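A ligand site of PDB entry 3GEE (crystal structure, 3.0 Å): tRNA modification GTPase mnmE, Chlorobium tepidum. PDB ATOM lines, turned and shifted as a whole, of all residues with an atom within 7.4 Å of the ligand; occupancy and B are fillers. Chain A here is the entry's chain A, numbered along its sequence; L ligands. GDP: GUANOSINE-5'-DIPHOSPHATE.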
ATOM      1  N   GLY A 240      27.412  33.031  -7.386  1.00  0.00           N
ATOM      2  CA  GLY A 240      26.095  32.595  -7.805  1.00  0.00           C
ATOM      3  C   GLY A 240      25.077  32.896  -6.726  1.00  0.00           C
ATOM      4  O   GLY A 240      25.423  32.972  -5.545  1.00  0.00           O
ATOM      5  N   LYS A 241      23.821  33.077  -7.126  1.00  0.00           N
ATOM      6  CA  LYS A 241      22.747  33.394  -6.192  1.00  0.00           C
ATOM      7  C   LYS A 241      22.340  32.161  -5.372  1.00  0.00           C
ATOM      8  O   LYS A 241      22.655  31.034  -5.766  1.00  0.00           O
ATOM      9  CB  LYS A 241      21.555  33.987  -6.941  1.00  0.00           C
ATOM     10  CG  LYS A 241      21.813  35.406  -7.430  1.00  0.00           C
ATOM     11  CD  LYS A 241      20.644  35.969  -8.206  1.00  0.00           C
ATOM     12  CE  LYS A 241      21.092  37.166  -9.040  1.00  0.00           C
ATOM     13  NZ  LYS A 241      20.103  37.524 -10.092  1.00  0.00           N
ATOM     14  N   PRO A 242      21.671  32.366  -4.217  1.00  0.00           N
ATOM     15  CA  PRO A 242      21.226  31.249  -3.380  1.00  0.00           C
ATOM     16  C   PRO A 242      20.582  30.112  -4.177  1.00  0.00           C
ATOM     17  O   PRO A 242      19.884  30.358  -5.173  1.00  0.00           O
ATOM     18  CB  PRO A 242      20.188  31.900  -2.467  1.00  0.00           C
ATOM     19  CG  PRO A 242      20.672  33.280  -2.302  1.00  0.00           C
ATOM     20  CD  PRO A 242      21.317  33.661  -3.605  1.00  0.00           C
ATOM     21  N   ASN A 243      20.837  28.875  -3.739  1.00  0.00           N
ATOM     22  CA  ASN A 243      20.278  27.653  -4.333  1.00  0.00           C
ATOM     23  C   ASN A 243      20.901  27.271  -5.682  1.00  0.00           C
ATOM     24  O   ASN A 243      20.412  26.371  -6.371  1.00  0.00           O
ATOM     25  CB  ASN A 243      18.745  27.742  -4.424  1.00  0.00           C
ATOM     26  CG  ASN A 243      18.074  26.395  -4.243  1.00  0.00           C
ATOM     27  OD1 ASN A 243      18.049  25.564  -5.148  1.00  0.00           O
ATOM     28  ND2 ASN A 243      17.487  26.169  -3.070  1.00  0.00           N
ATOM     29  N   ALA A 244      22.002  27.934  -6.048  1.00  0.00           N
ATOM     30  CA  ALA A 244      22.721  27.629  -7.282  1.00  0.00           C
ATOM     31  C   ALA A 244      23.381  26.257  -7.248  1.00  0.00           C
ATOM     32  O   ALA A 244      23.484  25.585  -8.280  1.00  0.00           O
ATOM     33  CB  ALA A 244      23.764  28.713  -7.571  1.00  0.00           C
ATOM     34  N   GLY A 245      23.840  25.845  -6.067  1.00  0.00           N
ATOM     35  CA  GLY A 245      24.555  24.576  -5.910  1.00  0.00           C
ATOM     36  C   GLY A 245      25.969  24.788  -5.387  1.00  0.00           C
ATOM     37  O   GLY A 245      26.797  23.874  -5.464  1.00  0.00           O
ATOM     38  N   LYS A 246      26.220  25.978  -4.847  1.00  0.00           N
ATOM     39  CA  LYS A 246      27.547  26.368  -4.372  1.00  0.00           C
ATOM     40  C   LYS A 246      28.087  25.405  -3.321  1.00  0.00           C
ATOM     41  O   LYS A 246      29.202  24.902  -3.442  1.00  0.00           O
ATOM     42  CB  LYS A 246      27.532  27.792  -3.818  1.00  0.00           C
ATOM     43  CG  LYS A 246      27.154  28.857  -4.844  1.00  0.00           C
ATOM     44  CD  LYS A 246      27.141  30.253  -4.247  1.00  0.00           C
ATOM     45  CE  LYS A 246      25.968  30.459  -3.295  1.00  0.00           C
ATOM     46  NZ  LYS A 246      25.761  31.884  -2.932  1.00  0.00           N
ATOM     47  N   SER A 247      27.279  25.141  -2.299  1.00  0.00           N
ATOM     48  CA  SER A 247      27.656  24.199  -1.242  1.00  0.00           C
ATOM     49  C   SER A 247      27.908  22.798  -1.809  1.00  0.00           C
ATOM     50  O   SER A 247      28.913  22.171  -1.477  1.00  0.00           O
ATOM     51  CB  SER A 247      26.583  24.172  -0.154  1.00  0.00           C
ATOM     52  OG  SER A 247      26.963  23.319   0.912  1.00  0.00           O
ATOM     53  N   THR A 248      27.008  22.348  -2.673  1.00  0.00           N
ATOM     54  CA  THR A 248      27.063  20.999  -3.268  1.00  0.00           C
ATOM     55  C   THR A 248      28.317  20.771  -4.100  1.00  0.00           C
ATOM     56  O   THR A 248      28.864  19.667  -4.110  1.00  0.00           O
ATOM     57  CB  THR A 248      25.815  20.705  -4.136  1.00  0.00           C
ATOM     58  OG1 THR A 248      24.638  21.160  -3.470  1.00  0.00           O
ATOM     59  CG2 THR A 248      25.693  19.213  -4.424  1.00  0.00           C
ATOM     60  N   LEU A 249      28.759  21.799  -4.814  1.00  0.00           N
ATOM     61  CA  LEU A 249      29.983  21.726  -5.613  1.00  0.00           C
ATOM     62  C   LEU A 249      31.187  21.673  -4.686  1.00  0.00           C
ATOM     63  O   LEU A 249      32.072  20.823  -4.842  1.00  0.00           O
ATOM     64  CB  LEU A 249      30.102  22.927  -6.542  1.00  0.00           C
ATOM     65  CG  LEU A 249      30.712  22.775  -7.940  1.00  0.00           C
ATOM     66  CD1 LEU A 249      31.407  24.063  -8.345  1.00  0.00           C
ATOM     67  CD2 LEU A 249      31.683  21.602  -8.081  1.00  0.00           C
ATOM     68  N   LEU A 250      31.196  22.583  -3.722  1.00  0.00           N
ATOM     69  CA  LEU A 250      32.310  22.767  -2.806  1.00  0.00           C
ATOM     70  C   LEU A 250      32.733  21.435  -2.180  1.00  0.00           C
ATOM     71  O   LEU A 250      33.888  21.024  -2.330  1.00  0.00           O
ATOM     72  CB  LEU A 250      31.932  23.793  -1.745  1.00  0.00           C
ATOM     73  CG  LEU A 250      33.048  24.585  -1.066  1.00  0.00           C
ATOM     74  CD1 LEU A 250      32.702  26.075  -1.012  1.00  0.00           C
ATOM     75  CD2 LEU A 250      33.356  24.034   0.322  1.00  0.00           C
ATOM     76  N   ASN A 251      31.805  20.760  -1.513  1.00  0.00           N
ATOM     77  CA  ASN A 251      32.128  19.518  -0.813  1.00  0.00           C
ATOM     78  C   ASN A 251      32.362  18.304  -1.720  1.00  0.00           C
ATOM     79  O   ASN A 251      32.929  17.299  -1.280  1.00  0.00           O
ATOM     80  CB  ASN A 251      31.076  19.213   0.269  1.00  0.00           C
ATOM     81  CG  ASN A 251      29.697  18.901  -0.298  1.00  0.00           C
ATOM     82  OD1 ASN A 251      29.381  19.269  -1.432  1.00  0.00           O
ATOM     83  ND2 ASN A 251      28.882  18.221   0.483  1.00  0.00           N
ATOM     84  N   LEU A 319      28.367  29.833 -10.678  1.00  0.00           N
ATOM     85  CA  LEU A 319      27.404  28.747 -10.699  1.00  0.00           C
ATOM     86  C   LEU A 319      26.006  29.276 -10.952  1.00  0.00           C
ATOM     87  O   LEU A 319      25.560  30.218 -10.293  1.00  0.00           O
ATOM     88  CB  LEU A 319      27.422  27.968  -9.391  1.00  0.00           C
ATOM     89  CG  LEU A 319      28.327  26.751  -9.260  1.00  0.00           C
ATOM     90  CD1 LEU A 319      28.305  26.271  -7.830  1.00  0.00           C
ATOM     91  CD2 LEU A 319      27.886  25.622 -10.182  1.00  0.00           C
ATOM     92  N   ASP A 321      22.030  27.456 -11.939  1.00  0.00           N
ATOM     93  CA  ASP A 321      21.333  26.189 -12.192  1.00  0.00           C
ATOM     94  C   ASP A 321      20.685  26.082 -13.583  1.00  0.00           C
ATOM     95  O   ASP A 321      19.616  26.633 -13.856  1.00  0.00           O
ATOM     96  CB  ASP A 321      20.397  25.727 -11.055  1.00  0.00           C
ATOM     97  CG  ASP A 321      19.553  26.843 -10.470  1.00  0.00           C
ATOM     98  OD1 ASP A 321      19.957  28.023 -10.543  1.00  0.00           O
ATOM     99  OD2 ASP A 321      18.482  26.530  -9.888  1.00  0.00           O
ATOM    100  N   ASN A 351      24.940  24.400 -13.461  1.00  0.00           N
ATOM    101  CA  ASN A 351      24.665  23.294 -12.548  1.00  0.00           C
ATOM    102  C   ASN A 351      23.309  22.625 -12.787  1.00  0.00           C
ATOM    103  O   ASN A 351      22.455  23.162 -13.508  1.00  0.00           O
ATOM    104  CB  ASN A 351      24.778  23.761 -11.090  1.00  0.00           C
ATOM    105  CG  ASN A 351      24.947  22.607 -10.112  1.00  0.00           C
ATOM    106  OD1 ASN A 351      25.441  21.530 -10.474  1.00  0.00           O
ATOM    107  ND2 ASN A 351      24.548  22.833  -8.868  1.00  0.00           N
ATOM    108  N   LYS A 352      23.115  21.442 -12.196  1.00  0.00           N
ATOM    109  CA  LYS A 352      21.861  20.691 -12.275  1.00  0.00           C
ATOM    110  C   LYS A 352      21.615  20.128 -13.687  1.00  0.00           C
ATOM    111  O   LYS A 352      20.493  20.151 -14.198  1.00  0.00           O
ATOM    112  CB  LYS A 352      20.668  21.528 -11.789  1.00  0.00           C
ATOM    113  CG  LYS A 352      20.771  21.987 -10.338  1.00  0.00           C
ATOM    114  CD  LYS A 352      19.453  22.546  -9.836  1.00  0.00           C
ATOM    115  CE  LYS A 352      19.482  22.832  -8.341  1.00  0.00           C
ATOM    116  NZ  LYS A 352      20.285  24.043  -8.007  1.00  0.00           N
ATOM    117  N   LEU A 353      22.680  19.622 -14.299  1.00  0.00           N
ATOM    118  CA  LEU A 353      22.632  19.019 -15.628  1.00  0.00           C
ATOM    119  C   LEU A 353      21.958  17.640 -15.624  1.00  0.00           C
ATOM    120  O   LEU A 353      21.522  17.152 -16.665  1.00  0.00           O
ATOM    121  CB  LEU A 353      24.053  18.920 -16.213  1.00  0.00           C
ATOM    122  CG  LEU A 353      24.332  18.187 -17.526  1.00  0.00           C
ATOM    123  CD1 LEU A 353      23.872  19.001 -18.728  1.00  0.00           C
ATOM    124  CD2 LEU A 353      25.809  17.837 -17.648  1.00  0.00           C
ATOM    125  N   ASP A 354      21.882  17.020 -14.448  1.00  0.00           N
ATOM    126  CA  ASP A 354      21.301  15.685 -14.316  1.00  0.00           C
ATOM    127  C   ASP A 354      19.820  15.609 -14.704  1.00  0.00           C
ATOM    128  O   ASP A 354      19.345  14.567 -15.145  1.00  0.00           O
ATOM    129  CB  ASP A 354      21.544  15.106 -12.909  1.00  0.00           C
ATOM    130  CG  ASP A 354      21.166  16.078 -11.799  1.00  0.00           C
ATOM    131  OD1 ASP A 354      19.957  16.211 -11.512  1.00  0.00           O
ATOM    132  OD2 ASP A 354      22.077  16.691 -11.213  1.00  0.00           O
ATOM    133  N   ARG A 355      19.105  16.718 -14.531  1.00  0.00           N
ATOM    134  CA  ARG A 355      17.734  16.846 -15.046  1.00  0.00           C
ATOM    135  C   ARG A 355      17.725  17.681 -16.329  1.00  0.00           C
ATOM    136  O   ARG A 355      18.680  18.414 -16.594  1.00  0.00           O
ATOM    137  CB  ARG A 355      16.772  17.414 -13.991  1.00  0.00           C
ATOM    138  CG  ARG A 355      16.803  18.938 -13.820  1.00  0.00           C
ATOM    139  CD  ARG A 355      17.732  19.384 -12.701  1.00  0.00           C
ATOM    140  NE  ARG A 355      17.284  18.925 -11.385  1.00  0.00           N
ATOM    141  CZ  ARG A 355      16.487  19.617 -10.569  1.00  0.00           C
ATOM    142  NH1 ARG A 355      16.133  19.103  -9.403  1.00  0.00           N
ATOM    143  NH2 ARG A 355      16.045  20.813 -10.924  1.00  0.00           N
ATOM    144  N   ILE A 377      27.447  20.904 -15.472  1.00  0.00           N
ATOM    145  CA  ILE A 377      27.812  20.278 -14.205  1.00  0.00           C
ATOM    146  C   ILE A 377      26.595  19.733 -13.474  1.00  0.00           C
ATOM    147  O   ILE A 377      25.545  20.371 -13.412  1.00  0.00           O
ATOM    148  CB  ILE A 377      28.585  21.284 -13.299  1.00  0.00           C
ATOM    149  CG1 ILE A 377      30.064  21.359 -13.703  1.00  0.00           C
ATOM    150  CG2 ILE A 377      28.448  20.949 -11.810  1.00  0.00           C
ATOM    151  CD1 ILE A 377      30.783  20.017 -13.711  1.00  0.00           C
ATOM    152  N   SER A 378      26.757  18.513 -12.959  1.00  0.00           N
ATOM    153  CA  SER A 378      25.849  17.978 -11.947  1.00  0.00           C
ATOM    154  C   SER A 378      26.656  17.862 -10.656  1.00  0.00           C
ATOM    155  O   SER A 378      27.398  16.904 -10.464  1.00  0.00           O
ATOM    156  CB  SER A 378      25.306  16.612 -12.366  1.00  0.00           C
ATOM    157  OG  SER A 378      24.571  16.023 -11.308  1.00  0.00           O
ATOM    158  N   ALA A 379      26.513  18.862  -9.795  1.00  0.00           N
ATOM    159  CA  ALA A 379      27.249  18.920  -8.527  1.00  0.00           C
ATOM    160  C   ALA A 379      26.831  17.819  -7.542  1.00  0.00           C
ATOM    161  O   ALA A 379      27.595  17.439  -6.666  1.00  0.00           O
ATOM    162  CB  ALA A 379      27.116  20.293  -7.883  1.00  0.00           C
ATOM    163  N   LEU A 380      25.612  17.315  -7.710  1.00  0.00           N
ATOM    164  CA  LEU A 380      25.086  16.257  -6.862  1.00  0.00           C
ATOM    165  C   LEU A 380      25.612  14.892  -7.306  1.00  0.00           C
ATOM    166  O   LEU A 380      26.182  14.147  -6.507  1.00  0.00           O
ATOM    167  CB  LEU A 380      23.556  16.270  -6.868  1.00  0.00           C
ATOM    168  CG  LEU A 380      22.770  15.675  -5.691  1.00  0.00           C
ATOM    169  CD1 LEU A 380      22.968  16.487  -4.417  1.00  0.00           C
ATOM    170  CD2 LEU A 380      21.294  15.592  -6.048  1.00  0.00           C
ATOM    171  N   ASN A 381      25.437  14.584  -8.591  1.00  0.00           N
ATOM    172  CA  ASN A 381      25.868  13.311  -9.174  1.00  0.00           C
ATOM    173  C   ASN A 381      27.384  13.263  -9.397  1.00  0.00           C
ATOM    174  O   ASN A 381      28.020  12.221  -9.195  1.00  0.00           O
ATOM    175  CB  ASN A 381      25.097  13.032 -10.470  1.00  0.00           C
ATOM    176  CG  ASN A 381      25.719  11.928 -11.305  1.00  0.00           C
ATOM    177  OD1 ASN A 381      26.196  12.182 -12.421  1.00  0.00           O
ATOM    178  ND2 ASN A 381      25.727  10.707 -10.784  1.00  0.00           N
ATOM    179  N   GLY A 382      27.954  14.398  -9.815  1.00  0.00           N
ATOM    180  CA  GLY A 382      29.367  14.492 -10.124  1.00  0.00           C
ATOM    181  C   GLY A 382      29.636  14.169 -11.586  1.00  0.00           C
ATOM    182  O   GLY A 382      30.371  13.231 -11.899  1.00  0.00           O
ATOM    183  N   ASP A 383      29.032  14.956 -12.473  1.00  0.00           N
ATOM    184  CA  ASP A 383      29.127  14.702 -13.912  1.00  0.00           C
ATOM    185  C   ASP A 383      29.729  15.907 -14.628  1.00  0.00           C
ATOM    186  O   ASP A 383      29.242  17.028 -14.488  1.00  0.00           O
ATOM    187  CB  ASP A 383      27.748  14.360 -14.487  1.00  0.00           C
ATOM    188  CG  ASP A 383      27.837  13.552 -15.775  1.00  0.00           C
ATOM    189  OD1 ASP A 383      27.262  12.440 -15.811  1.00  0.00           O
ATOM    190  OD2 ASP A 383      28.481  14.016 -16.738  1.00  0.00           O
HETATM  191  PB  GDP L   1      23.817  27.062  -2.250  1.00  0.00           P
HETATM  192  O1B GDP L   1      25.197  26.888  -1.679  1.00  0.00           O
HETATM  193  O2B GDP L   1      23.753  28.301  -3.107  1.00  0.00           O
HETATM  194  O3B GDP L   1      22.823  27.186  -1.112  1.00  0.00           O
HETATM  195  O3A GDP L   1      23.437  25.789  -3.143  1.00  0.00           O
HETATM  196  PA  GDP L   1      23.406  24.314  -2.503  1.00  0.00           P
HETATM  197  O1A GDP L   1      24.686  23.597  -2.812  1.00  0.00           O
HETATM  198  O2A GDP L   1      23.173  24.385  -1.013  1.00  0.00           O
HETATM  199  O5' GDP L   1      22.184  23.608  -3.255  1.00  0.00           O
HETATM  200  C5' GDP L   1      20.838  23.967  -2.946  1.00  0.00           C
HETATM  201  C4' GDP L   1      19.923  22.802  -3.272  1.00  0.00           C
HETATM  202  O4' GDP L   1      20.067  22.448  -4.658  1.00  0.00           O
HETATM  203  C3' GDP L   1      20.267  21.579  -2.449  1.00  0.00           C
HETATM  204  O3' GDP L   1      19.219  21.315  -1.507  1.00  0.00           O
HETATM  205  C2' GDP L   1      20.458  20.443  -3.447  1.00  0.00           C
HETATM  206  O2' GDP L   1      19.571  19.340  -3.188  1.00  0.00           O
HETATM  207  C1' GDP L   1      20.170  21.032  -4.819  1.00  0.00           C
HETATM  208  N9  GDP L   1      21.247  20.695  -5.777  1.00  0.00           N
HETATM  209  C8  GDP L   1      22.492  21.214  -5.763  1.00  0.00           C
HETATM  210  N7  GDP L   1      23.247  20.709  -6.769  1.00  0.00           N
HETATM  211  C5  GDP L   1      22.475  19.852  -7.460  1.00  0.00           C
HETATM  212  C6  GDP L   1      22.646  18.973  -8.646  1.00  0.00           C
HETATM  213  O6  GDP L   1      23.730  18.921  -9.265  1.00  0.00           O
HETATM  214  N1  GDP L   1      21.597  18.232  -9.040  1.00  0.00           N
HETATM  215  C2  GDP L   1      20.408  18.267  -8.403  1.00  0.00           C
HETATM  216  N2  GDP L   1      19.409  17.478  -8.867  1.00  0.00           N
HETATM  217  N3  GDP L   1      20.186  19.043  -7.304  1.00  0.00           N
HETATM  218  C4  GDP L   1      21.160  19.843  -6.803  1.00  0.00           C
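The side-chain amino group of Lys 246 is in hydrogen-bond range of the backbone carbonyl oxygen of Gly 240, at 2.9 Å. OD2 of Asp 321 is in salt-bridge range of NZ of Lys 352. The backbone carbonyl oxygen of Ser 378 sits at hydrogen-bond distance from the backbone NH of Asp 383, 3.2 Å away. NE of Arg 355 is in salt-bridge range of OD1 of Asp 354, 3.8 Å away. The backbone NH (N) of Lys 352 is in hydrogen-bond range of the backbone carbonyl oxygen (O) of Ile 377 (2.9 Å). The side-chain carboxylate of Asp 354 is in hydrogen-bond range of the side-chain hydroxyl of Ser 378, 2.6 Å away. The backbone carbonyl oxygen (O) of Thr 248 lies close to the side-chain amide oxygen (OD1) of Asn 251, 2.8 Å away. OD1 of Asn 351 lies close to O of Ile 377, at 3.2 Å.
Residues that only touch the ligand: Ser 378, Arg 355, Lys 352, Pro 242 and Lys 241. Hydrophobic or aromatic side chains that line the ligand: Ala 379 and Leu 380. The nearest printed residue that does not touch the ligand is Asn 381 (4.7 Å).
The side-chain carboxylate (OD2) of Asp 354 is in hydrogen-bond range of a nitrogen (N1) of the ligand (2.7 Å). The backbone NH (N) of Ser 247 sits at hydrogen-bond distance from an oxygen (O1B) of the ligand (2.8 Å). The side-chain hydroxyl (OG1) of Thr 248 lies within hydrogen-bond range of an oxygen (O1A) of the ligand (2.5 Å). The side-chain amide nitrogen of Asn 351 sits at hydrogen-bond distance from a nitrogen (N7) of the ligand, at 3.3 Å. The backbone NH (N) of Asn 243 sits at hydrogen-bond distance from an oxygen (O2B) of the ligand, 3.0 Å away. N of Lys 246 sits at hydrogen-bond distance from O3A of the ligand (3.3 Å). The backbone NH of Leu 380 sits at hydrogen-bond distance from an oxygen (O6) of the ligand, 2.9 Å away. N of Gly 245 is in hydrogen-bond range of O3A of the ligand (3.0 Å). N of Thr 248 lies within hydrogen-bond range of O1A of the ligand (2.6 Å). An oxygen (O2B) of the ligand sits at hydrogen-bond distance from the backbone NH (N) of Ala 244 (3.4 Å). An oxygen (O6) of the ligand sits at hydrogen-bond distance from the backbone NH of Ala 379 (2.8 Å).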
